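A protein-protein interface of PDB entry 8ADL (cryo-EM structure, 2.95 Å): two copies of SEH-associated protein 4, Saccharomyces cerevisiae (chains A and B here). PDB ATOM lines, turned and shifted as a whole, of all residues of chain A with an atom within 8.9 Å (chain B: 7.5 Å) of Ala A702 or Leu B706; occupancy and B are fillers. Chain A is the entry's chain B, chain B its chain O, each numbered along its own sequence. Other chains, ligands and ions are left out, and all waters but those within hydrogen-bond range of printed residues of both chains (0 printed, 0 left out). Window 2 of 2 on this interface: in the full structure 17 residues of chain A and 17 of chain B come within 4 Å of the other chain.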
ATOM      1  N   PRO A 676      -4.094 -15.211   1.076  1.00  0.00           N
ATOM      2  CA  PRO A 676      -4.429 -16.514   0.466  1.00  0.00           C
ATOM      3  C   PRO A 676      -3.271 -17.164  -0.273  1.00  0.00           C
ATOM      4  O   PRO A 676      -3.180 -18.399  -0.296  1.00  0.00           O
ATOM      5  CB  PRO A 676      -5.582 -16.169  -0.485  1.00  0.00           C
ATOM      6  CG  PRO A 676      -6.237 -15.030   0.161  1.00  0.00           C
ATOM      7  CD  PRO A 676      -5.107 -14.203   0.690  1.00  0.00           C
ATOM      8  N   ILE A 697      -3.485 -20.007   9.645  1.00  0.00           N
ATOM      9  CA  ILE A 697      -3.516 -18.805   8.813  1.00  0.00           C
ATOM     10  C   ILE A 697      -4.756 -18.790   7.921  1.00  0.00           C
ATOM     11  O   ILE A 697      -5.383 -17.743   7.719  1.00  0.00           O
ATOM     12  CB  ILE A 697      -2.224 -18.715   7.979  1.00  0.00           C
ATOM     13  CG1 ILE A 697      -1.010 -18.581   8.890  1.00  0.00           C
ATOM     14  CG2 ILE A 697      -2.258 -17.533   7.018  1.00  0.00           C
ATOM     15  CD1 ILE A 697       0.274 -18.972   8.209  1.00  0.00           C
ATOM     16  N   ALA A 698      -5.152 -19.960   7.411  1.00  0.00           N
ATOM     17  CA  ALA A 698      -6.383 -20.102   6.640  1.00  0.00           C
ATOM     18  C   ALA A 698      -7.634 -19.812   7.454  1.00  0.00           C
ATOM     19  O   ALA A 698      -8.671 -19.478   6.873  1.00  0.00           O
ATOM     20  CB  ALA A 698      -6.469 -21.510   6.048  1.00  0.00           C
ATOM     21  N   GLY A 699      -7.565 -19.922   8.777  1.00  0.00           N
ATOM     22  CA  GLY A 699      -8.688 -19.493   9.595  1.00  0.00           C
ATOM     23  C   GLY A 699      -8.821 -17.998   9.821  1.00  0.00           C
ATOM     24  O   GLY A 699      -9.319 -17.570  10.867  1.00  0.00           O
ATOM     25  N   TYR A 700      -8.415 -17.192   8.841  1.00  0.00           N
ATOM     26  CA  TYR A 700      -8.541 -15.744   8.905  1.00  0.00           C
ATOM     27  C   TYR A 700      -9.409 -15.146   7.806  1.00  0.00           C
ATOM     28  O   TYR A 700     -10.042 -14.114   8.046  1.00  0.00           O
ATOM     29  CB  TYR A 700      -7.139 -15.104   8.847  1.00  0.00           C
ATOM     30  CG  TYR A 700      -7.082 -13.687   8.313  1.00  0.00           C
ATOM     31  CD1 TYR A 700      -7.440 -12.608   9.115  1.00  0.00           C
ATOM     32  CD2 TYR A 700      -6.668 -13.425   7.009  1.00  0.00           C
ATOM     33  CE1 TYR A 700      -7.394 -11.313   8.634  1.00  0.00           C
ATOM     34  CE2 TYR A 700      -6.625 -12.135   6.522  1.00  0.00           C
ATOM     35  CZ  TYR A 700      -6.983 -11.083   7.337  1.00  0.00           C
ATOM     36  OH  TYR A 700      -6.934  -9.797   6.853  1.00  0.00           O
ATOM     37  N   LEU A 701      -9.471 -15.775   6.623  1.00  0.00           N
ATOM     38  CA  LEU A 701     -10.067 -15.136   5.450  1.00  0.00           C
ATOM     39  C   LEU A 701     -11.557 -14.862   5.635  1.00  0.00           C
ATOM     40  O   LEU A 701     -12.060 -13.817   5.208  1.00  0.00           O
ATOM     41  CB  LEU A 701      -9.837 -16.005   4.215  1.00  0.00           C
ATOM     42  CG  LEU A 701      -8.442 -16.618   4.071  1.00  0.00           C
ATOM     43  CD1 LEU A 701      -8.410 -17.616   2.923  1.00  0.00           C
ATOM     44  CD2 LEU A 701      -7.395 -15.533   3.870  1.00  0.00           C
ATOM     45  N   ALA A 702     -12.280 -15.787   6.260  1.00  0.00           N
ATOM     46  CA  ALA A 702     -13.671 -15.534   6.606  1.00  0.00           C
ATOM     47  C   ALA A 702     -13.821 -14.731   7.890  1.00  0.00           C
ATOM     48  O   ALA A 702     -14.929 -14.272   8.190  1.00  0.00           O
ATOM     49  CB  ALA A 702     -14.435 -16.849   6.731  1.00  0.00           C
ATOM     50  N   TYR A 703     -12.741 -14.553   8.646  1.00  0.00           N
ATOM     51  CA  TYR A 703     -12.773 -13.862   9.927  1.00  0.00           C
ATOM     52  C   TYR A 703     -12.513 -12.364   9.808  1.00  0.00           C
ATOM     53  O   TYR A 703     -12.766 -11.629  10.768  1.00  0.00           O
ATOM     54  CB  TYR A 703     -11.747 -14.508  10.870  1.00  0.00           C
ATOM     55  CG  TYR A 703     -11.805 -14.033  12.301  1.00  0.00           C
ATOM     56  CD1 TYR A 703     -12.801 -14.473  13.164  1.00  0.00           C
ATOM     57  CD2 TYR A 703     -10.858 -13.144  12.789  1.00  0.00           C
ATOM     58  CE1 TYR A 703     -12.852 -14.033  14.475  1.00  0.00           C
ATOM     59  CE2 TYR A 703     -10.900 -12.701  14.089  1.00  0.00           C
ATOM     60  CZ  TYR A 703     -11.895 -13.147  14.928  1.00  0.00           C
ATOM     61  OH  TYR A 703     -11.926 -12.697  16.224  1.00  0.00           O
ATOM     62  N   LYS A 704     -12.053 -11.890   8.646  1.00  0.00           N
ATOM     63  CA  LYS A 704     -11.671 -10.488   8.494  1.00  0.00           C
ATOM     64  C   LYS A 704     -12.861  -9.537   8.586  1.00  0.00           C
ATOM     65  O   LYS A 704     -12.666  -8.347   8.852  1.00  0.00           O
ATOM     66  CB  LYS A 704     -10.942 -10.287   7.165  1.00  0.00           C
ATOM     67  CG  LYS A 704     -11.787 -10.583   5.937  1.00  0.00           C
ATOM     68  CD  LYS A 704     -11.112 -10.098   4.667  1.00  0.00           C
ATOM     69  CE  LYS A 704     -11.996 -10.329   3.452  1.00  0.00           C
ATOM     70  NZ  LYS A 704     -12.377 -11.762   3.314  1.00  0.00           N
ATOM     71  N   ASP A 705     -14.080 -10.033   8.376  1.00  0.00           N
ATOM     72  CA  ASP A 705     -15.272  -9.208   8.515  1.00  0.00           C
ATOM     73  C   ASP A 705     -15.717  -9.056   9.963  1.00  0.00           C
ATOM     74  O   ASP A 705     -16.533  -8.174  10.255  1.00  0.00           O
ATOM     75  CB  ASP A 705     -16.414  -9.797   7.686  1.00  0.00           C
ATOM     76  CG  ASP A 705     -16.006 -10.083   6.253  1.00  0.00           C
ATOM     77  OD1 ASP A 705     -14.969  -9.547   5.812  1.00  0.00           O
ATOM     78  OD2 ASP A 705     -16.720 -10.846   5.571  1.00  0.00           O
ATOM     79  N   LEU A 706     -15.208  -9.890  10.870  1.00  0.00           N
ATOM     80  CA  LEU A 706     -15.639  -9.870  12.260  1.00  0.00           C
ATOM     81  C   LEU A 706     -15.048  -8.672  13.003  1.00  0.00           C
ATOM     82  O   LEU A 706     -13.941  -8.223  12.691  1.00  0.00           O
ATOM     83  CB  LEU A 706     -15.228 -11.161  12.967  1.00  0.00           C
ATOM     84  CG  LEU A 706     -16.153 -12.384  12.920  1.00  0.00           C
ATOM     85  CD1 LEU A 706     -17.505 -12.062  13.548  1.00  0.00           C
ATOM     86  CD2 LEU A 706     -16.322 -12.954  11.513  1.00  0.00           C
ATOM     87  N   PRO A 707     -15.782  -8.125  13.978  1.00  0.00           N
ATOM     88  CA  PRO A 707     -15.175  -7.142  14.893  1.00  0.00           C
ATOM     89  C   PRO A 707     -14.027  -7.705  15.711  1.00  0.00           C
ATOM     90  O   PRO A 707     -13.071  -6.978  16.008  1.00  0.00           O
ATOM     91  CB  PRO A 707     -16.350  -6.717  15.785  1.00  0.00           C
ATOM     92  CG  PRO A 707     -17.578  -7.084  15.013  1.00  0.00           C
ATOM     93  CD  PRO A 707     -17.218  -8.312  14.240  1.00  0.00           C
ATOM     94  N   TRP A 712     -10.159 -17.124  19.690  1.00  0.00           N
ATOM     95  CA  TRP A 712      -9.220 -17.462  18.627  1.00  0.00           C
ATOM     96  C   TRP A 712      -8.173 -16.371  18.427  1.00  0.00           C
ATOM     97  O   TRP A 712      -7.002 -16.671  18.162  1.00  0.00           O
ATOM     98  CB  TRP A 712      -9.991 -17.724  17.334  1.00  0.00           C
ATOM     99  CG  TRP A 712      -9.129 -18.005  16.153  1.00  0.00           C
ATOM    100  CD1 TRP A 712      -8.671 -19.220  15.738  1.00  0.00           C
ATOM    101  CD2 TRP A 712      -8.645 -17.049  15.207  1.00  0.00           C
ATOM    102  NE1 TRP A 712      -7.916 -19.077  14.600  1.00  0.00           N
ATOM    103  CE2 TRP A 712      -7.885 -17.752  14.254  1.00  0.00           C
ATOM    104  CE3 TRP A 712      -8.772 -15.663  15.079  1.00  0.00           C
ATOM    105  CZ2 TRP A 712      -7.257 -17.118  13.189  1.00  0.00           C
ATOM    106  CZ3 TRP A 712      -8.149 -15.037  14.023  1.00  0.00           C
ATOM    107  CH2 TRP A 712      -7.405 -15.763  13.090  1.00  0.00           C
ATOM    108  N   GLY B 699     -10.508 -21.911  14.959  1.00  0.00           N
ATOM    109  CA  GLY B 699     -10.854 -21.284  13.694  1.00  0.00           C
ATOM    110  C   GLY B 699     -12.156 -21.758  13.056  1.00  0.00           C
ATOM    111  O   GLY B 699     -12.372 -21.542  11.860  1.00  0.00           O
ATOM    112  N   TYR B 700     -13.025 -22.405  13.835  1.00  0.00           N
ATOM    113  CA  TYR B 700     -14.296 -22.950  13.372  1.00  0.00           C
ATOM    114  C   TYR B 700     -15.519 -22.240  13.937  1.00  0.00           C
ATOM    115  O   TYR B 700     -16.552 -22.197  13.264  1.00  0.00           O
ATOM    116  CB  TYR B 700     -14.365 -24.450  13.715  1.00  0.00           C
ATOM    117  CG  TYR B 700     -15.748 -25.056  13.873  1.00  0.00           C
ATOM    118  CD1 TYR B 700     -16.484 -25.459  12.766  1.00  0.00           C
ATOM    119  CD2 TYR B 700     -16.301 -25.255  15.136  1.00  0.00           C
ATOM    120  CE1 TYR B 700     -17.738 -26.023  12.910  1.00  0.00           C
ATOM    121  CE2 TYR B 700     -17.554 -25.815  15.288  1.00  0.00           C
ATOM    122  CZ  TYR B 700     -18.267 -26.198  14.173  1.00  0.00           C
ATOM    123  OH  TYR B 700     -19.515 -26.757  14.324  1.00  0.00           O
ATOM    124  N   ALA B 702     -16.243 -19.018  14.552  1.00  0.00           N
ATOM    125  CA  ALA B 702     -16.628 -17.913  13.687  1.00  0.00           C
ATOM    126  C   ALA B 702     -16.687 -18.310  12.216  1.00  0.00           C
ATOM    127  O   ALA B 702     -16.622 -17.436  11.345  1.00  0.00           O
ATOM    128  CB  ALA B 702     -15.667 -16.738  13.875  1.00  0.00           C
ATOM    129  N   TYR B 703     -16.807 -19.605  11.919  1.00  0.00           N
ATOM    130  CA  TYR B 703     -16.695 -20.093  10.553  1.00  0.00           C
ATOM    131  C   TYR B 703     -17.801 -21.057  10.137  1.00  0.00           C
ATOM    132  O   TYR B 703     -17.999 -21.245   8.930  1.00  0.00           O
ATOM    133  CB  TYR B 703     -15.333 -20.786  10.367  1.00  0.00           C
ATOM    134  CG  TYR B 703     -14.960 -21.114   8.943  1.00  0.00           C
ATOM    135  CD1 TYR B 703     -14.407 -20.146   8.119  1.00  0.00           C
ATOM    136  CD2 TYR B 703     -15.150 -22.389   8.422  1.00  0.00           C
ATOM    137  CE1 TYR B 703     -14.059 -20.431   6.817  1.00  0.00           C
ATOM    138  CE2 TYR B 703     -14.816 -22.679   7.116  1.00  0.00           C
ATOM    139  CZ  TYR B 703     -14.265 -21.697   6.324  1.00  0.00           C
ATOM    140  OH  TYR B 703     -13.917 -21.983   5.030  1.00  0.00           O
ATOM    141  N   LYS B 704     -18.564 -21.624  11.076  1.00  0.00           N
ATOM    142  CA  LYS B 704     -19.541 -22.668  10.772  1.00  0.00           C
ATOM    143  C   LYS B 704     -20.717 -22.195   9.922  1.00  0.00           C
ATOM    144  O   LYS B 704     -21.441 -23.039   9.385  1.00  0.00           O
ATOM    145  CB  LYS B 704     -20.075 -23.266  12.074  1.00  0.00           C
ATOM    146  CG  LYS B 704     -20.765 -22.254  12.972  1.00  0.00           C
ATOM    147  CD  LYS B 704     -21.357 -22.914  14.204  1.00  0.00           C
ATOM    148  CE  LYS B 704     -22.114 -21.905  15.051  1.00  0.00           C
ATOM    149  NZ  LYS B 704     -21.277 -20.717  15.373  1.00  0.00           N
ATOM    150  N   ASP B 705     -20.930 -20.887   9.784  1.00  0.00           N
ATOM    151  CA  ASP B 705     -21.988 -20.378   8.922  1.00  0.00           C
ATOM    152  C   ASP B 705     -21.599 -20.341   7.449  1.00  0.00           C
ATOM    153  O   ASP B 705     -22.459 -20.056   6.609  1.00  0.00           O
ATOM    154  CB  ASP B 705     -22.409 -18.979   9.380  1.00  0.00           C
ATOM    155  CG  ASP B 705     -22.883 -18.959  10.818  1.00  0.00           C
ATOM    156  OD1 ASP B 705     -23.325 -20.017  11.315  1.00  0.00           O
ATOM    157  OD2 ASP B 705     -22.814 -17.886  11.454  1.00  0.00           O
ATOM    158  N   LEU B 706     -20.336 -20.605   7.122  1.00  0.00           N
ATOM    159  CA  LEU B 706     -19.890 -20.573   5.735  1.00  0.00           C
ATOM    160  C   LEU B 706     -20.500 -21.737   4.953  1.00  0.00           C
ATOM    161  O   LEU B 706     -20.691 -22.824   5.509  1.00  0.00           O
ATOM    162  CB  LEU B 706     -18.363 -20.633   5.658  1.00  0.00           C
ATOM    163  CG  LEU B 706     -17.567 -19.320   5.648  1.00  0.00           C
ATOM    164  CD1 LEU B 706     -17.914 -18.475   4.431  1.00  0.00           C
ATOM    165  CD2 LEU B 706     -17.757 -18.519   6.933  1.00  0.00           C
ATOM    166  N   PRO B 707     -20.848 -21.527   3.677  1.00  0.00           N
ATOM    167  CA  PRO B 707     -21.472 -22.606   2.889  1.00  0.00           C
ATOM    168  C   PRO B 707     -20.590 -23.826   2.670  1.00  0.00           C
ATOM    169  O   PRO B 707     -21.112 -24.946   2.613  1.00  0.00           O
ATOM    170  CB  PRO B 707     -21.808 -21.916   1.558  1.00  0.00           C
ATOM    171  CG  PRO B 707     -21.851 -20.459   1.878  1.00  0.00           C
ATOM    172  CD  PRO B 707     -20.817 -20.254   2.938  1.00  0.00           C
ATOM    173  N   GLY B 708     -19.280 -23.655   2.546  1.00  0.00           N
ATOM    174  CA  GLY B 708     -18.379 -24.776   2.370  1.00  0.00           C
ATOM    175  C   GLY B 708     -17.593 -24.668   1.081  1.00  0.00           C
ATOM    176  O   GLY B 708     -17.640 -23.659   0.371  1.00  0.00           O
ATOM    177  N   ASN B 709     -16.857 -25.750   0.785  1.00  0.00           N
ATOM    178  CA  ASN B 709     -15.982 -25.866  -0.391  1.00  0.00           C
ATOM    179  C   ASN B 709     -14.955 -24.736  -0.449  1.00  0.00           C
ATOM    180  O   ASN B 709     -14.681 -24.173  -1.511  1.00  0.00           O
ATOM    181  CB  ASN B 709     -16.792 -25.936  -1.690  1.00  0.00           C
ATOM    182  CG  ASN B 709     -17.341 -27.323  -1.959  1.00  0.00           C
ATOM    183  OD1 ASN B 709     -16.625 -28.319  -1.850  1.00  0.00           O
ATOM    184  ND2 ASN B 709     -18.618 -27.396  -2.317  1.00  0.00           N
ATOM    185  N   ASN B 710     -14.386 -24.405   0.702  1.00  0.00           N
ATOM    186  CA  ASN B 710     -13.391 -23.352   0.831  1.00  0.00           C
ATOM    187  C   ASN B 710     -12.056 -23.966   1.241  1.00  0.00           C
ATOM    188  O   ASN B 710     -11.969 -25.151   1.578  1.00  0.00           O
ATOM    189  CB  ASN B 710     -13.863 -22.305   1.847  1.00  0.00           C
ATOM    190  CG  ASN B 710     -13.145 -20.975   1.710  1.00  0.00           C
ATOM    191  OD1 ASN B 710     -12.248 -20.823   0.881  1.00  0.00           O
ATOM    192  ND2 ASN B 710     -13.536 -20.007   2.528  1.00  0.00           N
ATOM    193  N   TRP B 712     -10.111 -23.482   3.809  1.00  0.00           N
ATOM    194  CA  TRP B 712      -9.966 -23.893   5.203  1.00  0.00           C
ATOM    195  C   TRP B 712     -10.536 -25.284   5.443  1.00  0.00           C
ATOM    196  O   TRP B 712      -9.916 -26.107   6.131  1.00  0.00           O
ATOM    197  CB  TRP B 712     -10.638 -22.877   6.118  1.00  0.00           C
ATOM    198  CG  TRP B 712     -10.320 -23.078   7.554  1.00  0.00           C
ATOM    199  CD1 TRP B 712      -9.253 -22.581   8.228  1.00  0.00           C
ATOM    200  CD2 TRP B 712     -11.097 -23.802   8.511  1.00  0.00           C
ATOM    201  NE1 TRP B 712      -9.301 -22.958   9.546  1.00  0.00           N
ATOM    202  CE2 TRP B 712     -10.428 -23.711   9.745  1.00  0.00           C
ATOM    203  CE3 TRP B 712     -12.285 -24.530   8.442  1.00  0.00           C
ATOM    204  CZ2 TRP B 712     -10.909 -24.313  10.897  1.00  0.00           C
ATOM    205  CZ3 TRP B 712     -12.764 -25.123   9.589  1.00  0.00           C
ATOM    206  CH2 TRP B 712     -12.077 -25.010  10.799  1.00  0.00           C
ATOM    207  N   ARG B 713     -11.705 -25.572   4.870  1.00  0.00           N
ATOM    208  CA  ARG B 713     -12.270 -26.909   4.986  1.00  0.00           C
ATOM    209  C   ARG B 713     -11.449 -27.926   4.208  1.00  0.00           C
ATOM    210  O   ARG B 713     -11.334 -29.081   4.634  1.00  0.00           O
ATOM    211  CB  ARG B 713     -13.721 -26.892   4.512  1.00  0.00           C
ATOM    212  CG  ARG B 713     -14.648 -26.148   5.463  1.00  0.00           C
ATOM    213  CD  ARG B 713     -16.111 -26.435   5.178  1.00  0.00           C
ATOM    214  NE  ARG B 713     -16.950 -25.271   5.430  1.00  0.00           N
ATOM    215  CZ  ARG B 713     -17.433 -24.937   6.619  1.00  0.00           C
ATOM    216  NH1 ARG B 713     -17.164 -25.654   7.699  1.00  0.00           N
ATOM    217  NH2 ARG B 713     -18.198 -23.857   6.731  1.00  0.00           N
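O of Tyr B703 sits at hydrogen-bond distance from NH2 of Arg B713 (3.4 Å). The backbone carbonyl oxygen of Leu B706 sits at hydrogen-bond distance from the guanidinium group of Arg B713. The side-chain hydroxyl (OH) of Tyr B703 lies close to the side-chain amide nitrogen (ND2) of Asn B710 (3.2 Å).
Of the 13 printed residues of chain A, 5 touch a printed residue of chain B. Hydrophobic or aromatic side chains of chain A that line the printed part of chain B: Ala A698, Ala A702, Tyr A703 and Trp A712. Among the printed residues, 6 pairs touch across the chains. Among the printed residues, no Asp or Glu carboxylate lies within 4 Å of a Lys or Arg side-chain nitrogen of the other chain.
Ala A702 touches two residues of chain B. Leu B706 touches just one residue of chain A: Ala A702 (3.7 Å). Pro B707 touches none of the printed residues of chain A. Of the printed residues of chain B, Trp A712 touches Gly B699 (3.4 Å). Of the printed residues of chain B, Gly A699 touches Trp B712 (3.2 Å).
Gly A699 touches Trp B712, and with the chains exchanged Trp A712 touches Gly B699. Ala A702 touches Tyr B703, and with the chains exchanged Tyr A703 touches Ala B702. Ala A702 touches Leu B706, but with the chains exchanged Leu A706 does not touch Ala B702 (4.5 Å). Of the 6 pairs that touch across the chains among the printed residues, 4 have their exchanged pair printed and touching as well.
Ala A698 touches Trp B712 (C to CD1, 3.3 Å). Gly A699 touches Trp B712 (N to CD1, 3.2 Å). Tyr B703 touches Ala A702 (CD1 to CB, 3.6 Å). Ala A702 touches Leu B706. CB of Ala B702 touches CD1 of Tyr A703, at 3.7 Å. Gly B699 touches Trp A712 (N to CD1, 3.4 Å).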
